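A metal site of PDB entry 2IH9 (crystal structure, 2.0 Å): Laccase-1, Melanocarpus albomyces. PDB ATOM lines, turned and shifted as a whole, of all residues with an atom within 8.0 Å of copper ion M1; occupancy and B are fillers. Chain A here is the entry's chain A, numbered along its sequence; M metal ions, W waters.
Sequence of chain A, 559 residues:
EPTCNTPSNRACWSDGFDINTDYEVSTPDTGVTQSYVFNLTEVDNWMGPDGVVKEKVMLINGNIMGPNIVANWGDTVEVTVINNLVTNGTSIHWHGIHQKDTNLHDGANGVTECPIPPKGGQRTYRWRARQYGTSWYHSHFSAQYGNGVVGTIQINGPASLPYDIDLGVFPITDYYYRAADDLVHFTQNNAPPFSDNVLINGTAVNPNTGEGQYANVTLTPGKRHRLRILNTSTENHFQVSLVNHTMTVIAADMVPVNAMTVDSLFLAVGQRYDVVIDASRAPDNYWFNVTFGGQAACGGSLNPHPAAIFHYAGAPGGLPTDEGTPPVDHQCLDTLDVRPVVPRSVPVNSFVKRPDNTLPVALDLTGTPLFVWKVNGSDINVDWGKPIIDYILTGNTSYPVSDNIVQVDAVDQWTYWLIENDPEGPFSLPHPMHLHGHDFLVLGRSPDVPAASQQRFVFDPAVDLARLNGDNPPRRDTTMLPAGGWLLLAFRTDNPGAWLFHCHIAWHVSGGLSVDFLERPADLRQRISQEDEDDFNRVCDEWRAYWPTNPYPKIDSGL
NE2 of His 95 sits close to NH1 of Arg 272 (3.3 Å).
The backbone carbonyl oxygen of Trp 136 lies within hydrogen-bond range of the backbone NH of His 95 (3.0 Å).
NE2 of His 95 sits at hydrogen-bond distance from O of Gly 270.
A ring nitrogen (NE2) of His 95 is in hydrogen-bond range of the side-chain carboxylate (OD1) of Asp 477 (3.2 Å).
N of His 93 is in hydrogen-bond range of O of His 138 (2.8 Å).
A ring nitrogen (ND1) of His 504 lies within hydrogen-bond range of the side-chain hydroxyl of Tyr 145, at 3.2 Å.
Merely in contact with copper ion M1: His 93 and Trp 136.
Five residues have an atom within 4 Å of copper ion M1: His 93, His 95, Trp 136, His 138 and His 504.
Along chain A the residues within 4 Å of copper ion M1 span positions 93 to 504.
Copper ion M1 is bound by a ring nitrogen (NE2) of His 138 (1.9 Å), a ring nitrogen (ND1) of His 95 (1.9 Å), a ring nitrogen (NE2) of His 504 (2.0 Å) and water W1 (2.3 Å).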
ATOM      1  N   HIS A  93     -21.828  22.989  13.453  1.00  0.00           N
ATOM      2  CA  HIS A  93     -20.915  24.053  13.063  1.00  0.00           C
ATOM      3  C   HIS A  93     -19.645  23.906  13.852  1.00  0.00           C
ATOM      4  O   HIS A  93     -19.676  23.777  15.064  1.00  0.00           O
ATOM      5  CB  HIS A  93     -21.551  25.432  13.289  1.00  0.00           C
ATOM      6  CG  HIS A  93     -20.615  26.587  13.045  1.00  0.00           C
ATOM      7  ND1 HIS A  93     -19.831  26.679  11.918  1.00  0.00           N
ATOM      8  CD2 HIS A  93     -20.295  27.645  13.813  1.00  0.00           C
ATOM      9  CE1 HIS A  93     -19.062  27.745  12.011  1.00  0.00           C
ATOM     10  NE2 HIS A  93     -19.326  28.350  13.144  1.00  0.00           N
ATOM     11  N   TRP A  94     -18.533  23.954  13.122  1.00  0.00           N
ATOM     12  CA  TRP A  94     -17.184  23.818  13.687  1.00  0.00           C
ATOM     13  C   TRP A  94     -16.604  25.216  13.868  1.00  0.00           C
ATOM     14  O   TRP A  94     -15.834  25.691  13.040  1.00  0.00           O
ATOM     15  CB  TRP A  94     -16.321  22.918  12.774  1.00  0.00           C
ATOM     16  CG  TRP A  94     -17.090  21.739  12.228  1.00  0.00           C
ATOM     17  CD1 TRP A  94     -17.762  21.678  11.038  1.00  0.00           C
ATOM     18  CD2 TRP A  94     -17.395  20.524  12.921  1.00  0.00           C
ATOM     19  NE1 TRP A  94     -18.484  20.516  10.947  1.00  0.00           N
ATOM     20  CE2 TRP A  94     -18.284  19.785  12.087  1.00  0.00           C
ATOM     21  CE3 TRP A  94     -17.030  19.981  14.175  1.00  0.00           C
ATOM     22  CZ2 TRP A  94     -18.809  18.537  12.472  1.00  0.00           C
ATOM     23  CZ3 TRP A  94     -17.556  18.734  14.560  1.00  0.00           C
ATOM     24  CH2 TRP A  94     -18.436  18.018  13.707  1.00  0.00           C
ATOM     25  N   HIS A  95     -17.031  25.856  14.963  1.00  0.00           N
ATOM     26  CA  HIS A  95     -16.649  27.215  15.361  1.00  0.00           C
ATOM     27  C   HIS A  95     -15.137  27.343  15.569  1.00  0.00           C
ATOM     28  O   HIS A  95     -14.577  26.752  16.485  1.00  0.00           O
ATOM     29  CB  HIS A  95     -17.421  27.583  16.649  1.00  0.00           C
ATOM     30  CG  HIS A  95     -17.307  29.012  17.091  1.00  0.00           C
ATOM     31  ND1 HIS A  95     -18.388  29.725  17.583  1.00  0.00           N
ATOM     32  CD2 HIS A  95     -16.229  29.841  17.225  1.00  0.00           C
ATOM     33  CE1 HIS A  95     -17.975  30.914  18.000  1.00  0.00           C
ATOM     34  NE2 HIS A  95     -16.675  31.004  17.799  1.00  0.00           N
ATOM     35  N   GLY A  96     -14.525  28.196  14.757  1.00  0.00           N
ATOM     36  CA  GLY A  96     -13.094  28.414  14.833  1.00  0.00           C
ATOM     37  C   GLY A  96     -12.374  27.894  13.615  1.00  0.00           C
ATOM     38  O   GLY A  96     -11.378  28.467  13.177  1.00  0.00           O
ATOM     39  N   TRP A 136     -14.378  25.000  19.374  1.00  0.00           N
ATOM     40  CA  TRP A 136     -15.539  24.228  19.803  1.00  0.00           C
ATOM     41  C   TRP A 136     -16.502  24.035  18.669  1.00  0.00           C
ATOM     42  O   TRP A 136     -16.324  24.596  17.582  1.00  0.00           O
ATOM     43  CB  TRP A 136     -16.241  24.892  21.016  1.00  0.00           C
ATOM     44  CG  TRP A 136     -16.872  26.253  20.774  1.00  0.00           C
ATOM     45  CD1 TRP A 136     -16.249  27.391  20.332  1.00  0.00           C
ATOM     46  CD2 TRP A 136     -18.221  26.631  21.071  1.00  0.00           C
ATOM     47  NE1 TRP A 136     -17.110  28.449  20.345  1.00  0.00           N
ATOM     48  CE2 TRP A 136     -18.332  28.021  20.797  1.00  0.00           C
ATOM     49  CE3 TRP A 136     -19.343  25.933  21.563  1.00  0.00           C
ATOM     50  CZ2 TRP A 136     -19.533  28.737  20.999  1.00  0.00           C
ATOM     51  CZ3 TRP A 136     -20.555  26.656  21.765  1.00  0.00           C
ATOM     52  CH2 TRP A 136     -20.633  28.046  21.483  1.00  0.00           C
ATOM     53  N   TYR A 137     -17.471  23.163  18.905  1.00  0.00           N
ATOM     54  CA  TYR A 137     -18.506  22.892  17.927  1.00  0.00           C
ATOM     55  C   TYR A 137     -19.884  22.992  18.577  1.00  0.00           C
ATOM     56  O   TYR A 137     -20.005  22.879  19.804  1.00  0.00           O
ATOM     57  CB  TYR A 137     -18.288  21.546  17.220  1.00  0.00           C
ATOM     58  CG  TYR A 137     -18.267  20.306  18.101  1.00  0.00           C
ATOM     59  CD1 TYR A 137     -19.458  19.654  18.469  1.00  0.00           C
ATOM     60  CD2 TYR A 137     -17.035  19.758  18.541  1.00  0.00           C
ATOM     61  CE1 TYR A 137     -19.436  18.490  19.273  1.00  0.00           C
ATOM     62  CE2 TYR A 137     -17.008  18.589  19.339  1.00  0.00           C
ATOM     63  CZ  TYR A 137     -18.213  17.967  19.698  1.00  0.00           C
ATOM     64  OH  TYR A 137     -18.207  16.841  20.454  1.00  0.00           O
ATOM     65  N   HIS A 138     -20.917  23.189  17.759  1.00  0.00           N
ATOM     66  CA  HIS A 138     -22.295  23.322  18.250  1.00  0.00           C
ATOM     67  C   HIS A 138     -23.313  23.277  17.103  1.00  0.00           C
ATOM     68  O   HIS A 138     -22.949  23.489  15.944  1.00  0.00           O
ATOM     69  CB  HIS A 138     -22.456  24.628  19.051  1.00  0.00           C
ATOM     70  CG  HIS A 138     -22.168  25.878  18.279  1.00  0.00           C
ATOM     71  ND1 HIS A 138     -23.099  26.499  17.469  1.00  0.00           N
ATOM     72  CD2 HIS A 138     -21.055  26.651  18.209  1.00  0.00           C
ATOM     73  CE1 HIS A 138     -22.575  27.588  16.960  1.00  0.00           C
ATOM     74  NE2 HIS A 138     -21.337  27.716  17.387  1.00  0.00           N
ATOM     75  N   SER A 139     -24.588  23.049  17.443  1.00  0.00           N
ATOM     76  CA  SER A 139     -25.650  23.042  16.432  1.00  0.00           C
ATOM     77  C   SER A 139     -25.956  24.481  16.007  1.00  0.00           C
ATOM     78  O   SER A 139     -25.641  25.439  16.729  1.00  0.00           O
ATOM     79  CB  SER A 139     -26.929  22.403  16.962  1.00  0.00           C
ATOM     80  OG  SER A 139     -27.971  22.390  15.987  1.00  0.00           O
ATOM     81  N   HIS A 140     -26.523  24.629  14.820  1.00  0.00           N
ATOM     82  CA  HIS A 140     -26.878  25.939  14.316  1.00  0.00           C
ATOM     83  C   HIS A 140     -28.363  25.952  13.939  1.00  0.00           C
ATOM     84  O   HIS A 140     -28.835  26.915  13.355  1.00  0.00           O
ATOM     85  CB  HIS A 140     -25.969  26.348  13.147  1.00  0.00           C
ATOM     86  CG  HIS A 140     -25.359  27.713  13.303  1.00  0.00           C
ATOM     87  ND1 HIS A 140     -26.093  28.818  13.657  1.00  0.00           N
ATOM     88  CD2 HIS A 140     -24.075  28.140  13.194  1.00  0.00           C
ATOM     89  CE1 HIS A 140     -25.295  29.864  13.774  1.00  0.00           C
ATOM     90  NE2 HIS A 140     -24.055  29.475  13.492  1.00  0.00           N
ATOM     91  N   TYR A 145     -28.373  24.274  20.391  1.00  0.00           N
ATOM     92  CA  TYR A 145     -27.166  24.071  21.193  1.00  0.00           C
ATOM     93  C   TYR A 145     -27.344  24.369  22.695  1.00  0.00           C
ATOM     94  O   TYR A 145     -26.565  23.902  23.528  1.00  0.00           O
ATOM     95  CB  TYR A 145     -25.929  24.747  20.535  1.00  0.00           C
ATOM     96  CG  TYR A 145     -25.567  26.191  20.896  1.00  0.00           C
ATOM     97  CD1 TYR A 145     -24.686  26.475  21.976  1.00  0.00           C
ATOM     98  CD2 TYR A 145     -26.025  27.273  20.109  1.00  0.00           C
ATOM     99  CE1 TYR A 145     -24.261  27.807  22.257  1.00  0.00           C
ATOM    100  CE2 TYR A 145     -25.615  28.607  20.377  1.00  0.00           C
ATOM    101  CZ  TYR A 145     -24.733  28.855  21.463  1.00  0.00           C
ATOM    102  OH  TYR A 145     -24.354  30.130  21.753  1.00  0.00           O
ATOM    103  N   ASN A 231     -15.835  29.595  26.460  1.00  0.00           N
ATOM    104  CA  ASN A 231     -17.134  30.103  26.865  1.00  0.00           C
ATOM    105  C   ASN A 231     -18.113  29.529  25.835  1.00  0.00           C
ATOM    106  O   ASN A 231     -18.281  30.079  24.741  1.00  0.00           O
ATOM    107  CB  ASN A 231     -17.181  31.637  26.886  1.00  0.00           C
ATOM    108  CG  ASN A 231     -18.506  32.174  27.433  1.00  0.00           C
ATOM    109  OD1 ASN A 231     -19.451  31.416  27.667  1.00  0.00           O
ATOM    110  ND2 ASN A 231     -18.580  33.479  27.633  1.00  0.00           N
ATOM    111  N   SER A 233     -21.406  29.275  26.241  1.00  0.00           N
ATOM    112  CA  SER A 233     -22.742  29.788  26.583  1.00  0.00           C
ATOM    113  C   SER A 233     -23.654  30.199  25.431  1.00  0.00           C
ATOM    114  O   SER A 233     -23.210  30.302  24.295  1.00  0.00           O
ATOM    115  CB  SER A 233     -22.590  31.019  27.487  1.00  0.00           C
ATOM    116  OG  SER A 233     -22.137  30.688  28.779  1.00  0.00           O
ATOM    117  N   VAL A 269     -19.257  35.297  24.568  1.00  0.00           N
ATOM    118  CA  VAL A 269     -19.838  34.032  24.096  1.00  0.00           C
ATOM    119  C   VAL A 269     -19.048  33.629  22.840  1.00  0.00           C
ATOM    120  O   VAL A 269     -18.796  34.461  21.958  1.00  0.00           O
ATOM    121  CB  VAL A 269     -21.340  34.174  23.767  1.00  0.00           C
ATOM    122  CG1 VAL A 269     -21.903  32.870  23.221  1.00  0.00           C
ATOM    123  CG2 VAL A 269     -22.112  34.566  25.000  1.00  0.00           C
ATOM    124  N   GLY A 270     -18.544  32.390  22.855  1.00  0.00           N
ATOM    125  CA  GLY A 270     -17.782  31.872  21.743  1.00  0.00           C
ATOM    126  C   GLY A 270     -16.271  32.095  21.806  1.00  0.00           C
ATOM    127  O   GLY A 270     -15.522  31.527  21.002  1.00  0.00           O
ATOM    128  N   GLN A 271     -15.829  32.931  22.754  1.00  0.00           N
ATOM    129  CA  GLN A 271     -14.407  33.229  22.918  1.00  0.00           C
ATOM    130  C   GLN A 271     -13.653  32.158  23.678  1.00  0.00           C
ATOM    131  O   GLN A 271     -14.239  31.407  24.468  1.00  0.00           O
ATOM    132  CB  GLN A 271     -14.191  34.577  23.606  1.00  0.00           C
ATOM    133  CG  GLN A 271     -14.279  35.740  22.647  1.00  0.00           C
ATOM    134  CD  GLN A 271     -13.811  37.067  23.215  1.00  0.00           C
ATOM    135  OE1 GLN A 271     -13.726  37.255  24.425  1.00  0.00           O
ATOM    136  NE2 GLN A 271     -13.536  37.999  22.327  1.00  0.00           N
ATOM    137  N   ARG A 272     -12.361  32.039  23.350  1.00  0.00           N
ATOM    138  CA  ARG A 272     -11.451  31.074  23.986  1.00  0.00           C
ATOM    139  C   ARG A 272     -10.124  31.745  24.309  1.00  0.00           C
ATOM    140  O   ARG A 272      -9.711  32.712  23.655  1.00  0.00           O
ATOM    141  CB  ARG A 272     -11.133  29.862  23.089  1.00  0.00           C
ATOM    142  CG  ARG A 272     -12.240  28.860  22.842  1.00  0.00           C
ATOM    143  CD  ARG A 272     -13.068  29.188  21.593  1.00  0.00           C
ATOM    144  NE  ARG A 272     -12.286  29.082  20.364  1.00  0.00           N
ATOM    145  CZ  ARG A 272     -12.586  29.702  19.236  1.00  0.00           C
ATOM    146  NH1 ARG A 272     -13.660  30.485  19.158  1.00  0.00           N
ATOM    147  NH2 ARG A 272     -11.816  29.543  18.162  1.00  0.00           N
ATOM    148  N   HIS A 434     -19.370  37.394  15.860  1.00  0.00           N
ATOM    149  CA  HIS A 434     -18.617  36.262  15.357  1.00  0.00           C
ATOM    150  C   HIS A 434     -18.679  36.166  13.835  1.00  0.00           C
ATOM    151  O   HIS A 434     -19.729  36.420  13.248  1.00  0.00           O
ATOM    152  CB  HIS A 434     -19.174  34.961  15.995  1.00  0.00           C
ATOM    153  CG  HIS A 434     -18.617  33.696  15.395  1.00  0.00           C
ATOM    154  ND1 HIS A 434     -17.264  33.445  15.289  1.00  0.00           N
ATOM    155  CD2 HIS A 434     -19.247  32.636  14.825  1.00  0.00           C
ATOM    156  CE1 HIS A 434     -17.084  32.289  14.666  1.00  0.00           C
ATOM    157  NE2 HIS A 434     -18.267  31.786  14.370  1.00  0.00           N
ATOM    158  N   HIS A 436     -17.885  33.544  10.505  1.00  0.00           N
ATOM    159  CA  HIS A 436     -17.623  32.182  10.019  1.00  0.00           C
ATOM    160  C   HIS A 436     -16.568  32.273   8.907  1.00  0.00           C
ATOM    161  O   HIS A 436     -16.442  33.307   8.241  1.00  0.00           O
ATOM    162  CB  HIS A 436     -18.888  31.520   9.447  1.00  0.00           C
ATOM    163  CG  HIS A 436     -19.902  31.090  10.470  1.00  0.00           C
ATOM    164  ND1 HIS A 436     -20.743  30.016  10.273  1.00  0.00           N
ATOM    165  CD2 HIS A 436     -20.260  31.632  11.664  1.00  0.00           C
ATOM    166  CE1 HIS A 436     -21.575  29.913  11.299  1.00  0.00           C
ATOM    167  NE2 HIS A 436     -21.300  30.880  12.158  1.00  0.00           N
ATOM    168  N   ASP A 477     -11.783  35.157  16.019  1.00  0.00           N
ATOM    169  CA  ASP A 477     -13.075  34.954  15.362  1.00  0.00           C
ATOM    170  C   ASP A 477     -14.293  35.554  16.062  1.00  0.00           C
ATOM    171  O   ASP A 477     -15.385  35.565  15.485  1.00  0.00           O
ATOM    172  CB  ASP A 477     -13.303  33.457  15.020  1.00  0.00           C
ATOM    173  CG  ASP A 477     -13.413  32.553  16.261  1.00  0.00           C
ATOM    174  OD1 ASP A 477     -14.198  32.852  17.183  1.00  0.00           O
ATOM    175  OD2 ASP A 477     -12.733  31.518  16.288  1.00  0.00           O
ATOM    176  N   THR A 478     -14.107  36.073  17.277  1.00  0.00           N
ATOM    177  CA  THR A 478     -15.186  36.681  18.065  1.00  0.00           C
ATOM    178  C   THR A 478     -14.693  37.873  18.880  1.00  0.00           C
ATOM    179  O   THR A 478     -13.702  37.764  19.612  1.00  0.00           O
ATOM    180  CB  THR A 478     -15.811  35.659  19.084  1.00  0.00           C
ATOM    181  OG1 THR A 478     -16.143  34.432  18.431  1.00  0.00           O
ATOM    182  CG2 THR A 478     -17.058  36.239  19.736  1.00  0.00           C
ATOM    183  N   HIS A 502     -22.543  37.058  12.650  1.00  0.00           N
ATOM    184  CA  HIS A 502     -23.608  37.269  13.625  1.00  0.00           C
ATOM    185  C   HIS A 502     -23.203  37.484  15.061  1.00  0.00           C
ATOM    186  O   HIS A 502     -22.061  37.235  15.453  1.00  0.00           O
ATOM    187  CB  HIS A 502     -24.583  36.060  13.597  1.00  0.00           C
ATOM    188  CG  HIS A 502     -23.951  34.729  13.919  1.00  0.00           C
ATOM    189  ND1 HIS A 502     -23.979  34.181  15.190  1.00  0.00           N
ATOM    190  CD2 HIS A 502     -23.342  33.806  13.138  1.00  0.00           C
ATOM    191  CE1 HIS A 502     -23.419  32.988  15.167  1.00  0.00           C
ATOM    192  NE2 HIS A 502     -23.025  32.730  13.932  1.00  0.00           N
ATOM    193  N   HIS A 504     -23.356  36.182  18.688  1.00  0.00           N
ATOM    194  CA  HIS A 504     -23.433  34.807  19.148  1.00  0.00           C
ATOM    195  C   HIS A 504     -24.424  34.543  20.288  1.00  0.00           C
ATOM    196  O   HIS A 504     -24.557  33.390  20.723  1.00  0.00           O
ATOM    197  CB  HIS A 504     -22.036  34.261  19.478  1.00  0.00           C
ATOM    198  CG  HIS A 504     -21.845  32.821  19.101  1.00  0.00           C
ATOM    199  ND1 HIS A 504     -22.435  31.779  19.787  1.00  0.00           N
ATOM    200  CD2 HIS A 504     -21.078  32.250  18.140  1.00  0.00           C
ATOM    201  CE1 HIS A 504     -22.028  30.623  19.274  1.00  0.00           C
ATOM    202  NE2 HIS A 504     -21.193  30.885  18.279  1.00  0.00           N
HETATM  203 CU    CU M   1     -20.287  29.345  17.408  1.00  0.00          CU
HETATM  204 CU    CU M   2     -18.729  30.006  13.850  1.00  0.00          CU
HETATM  205 CU    CU M   3     -22.685  30.909  13.473  1.00  0.00          CU
HETATM  206  O   HOH W   1     -21.724  29.959  15.689  1.00  0.00           O
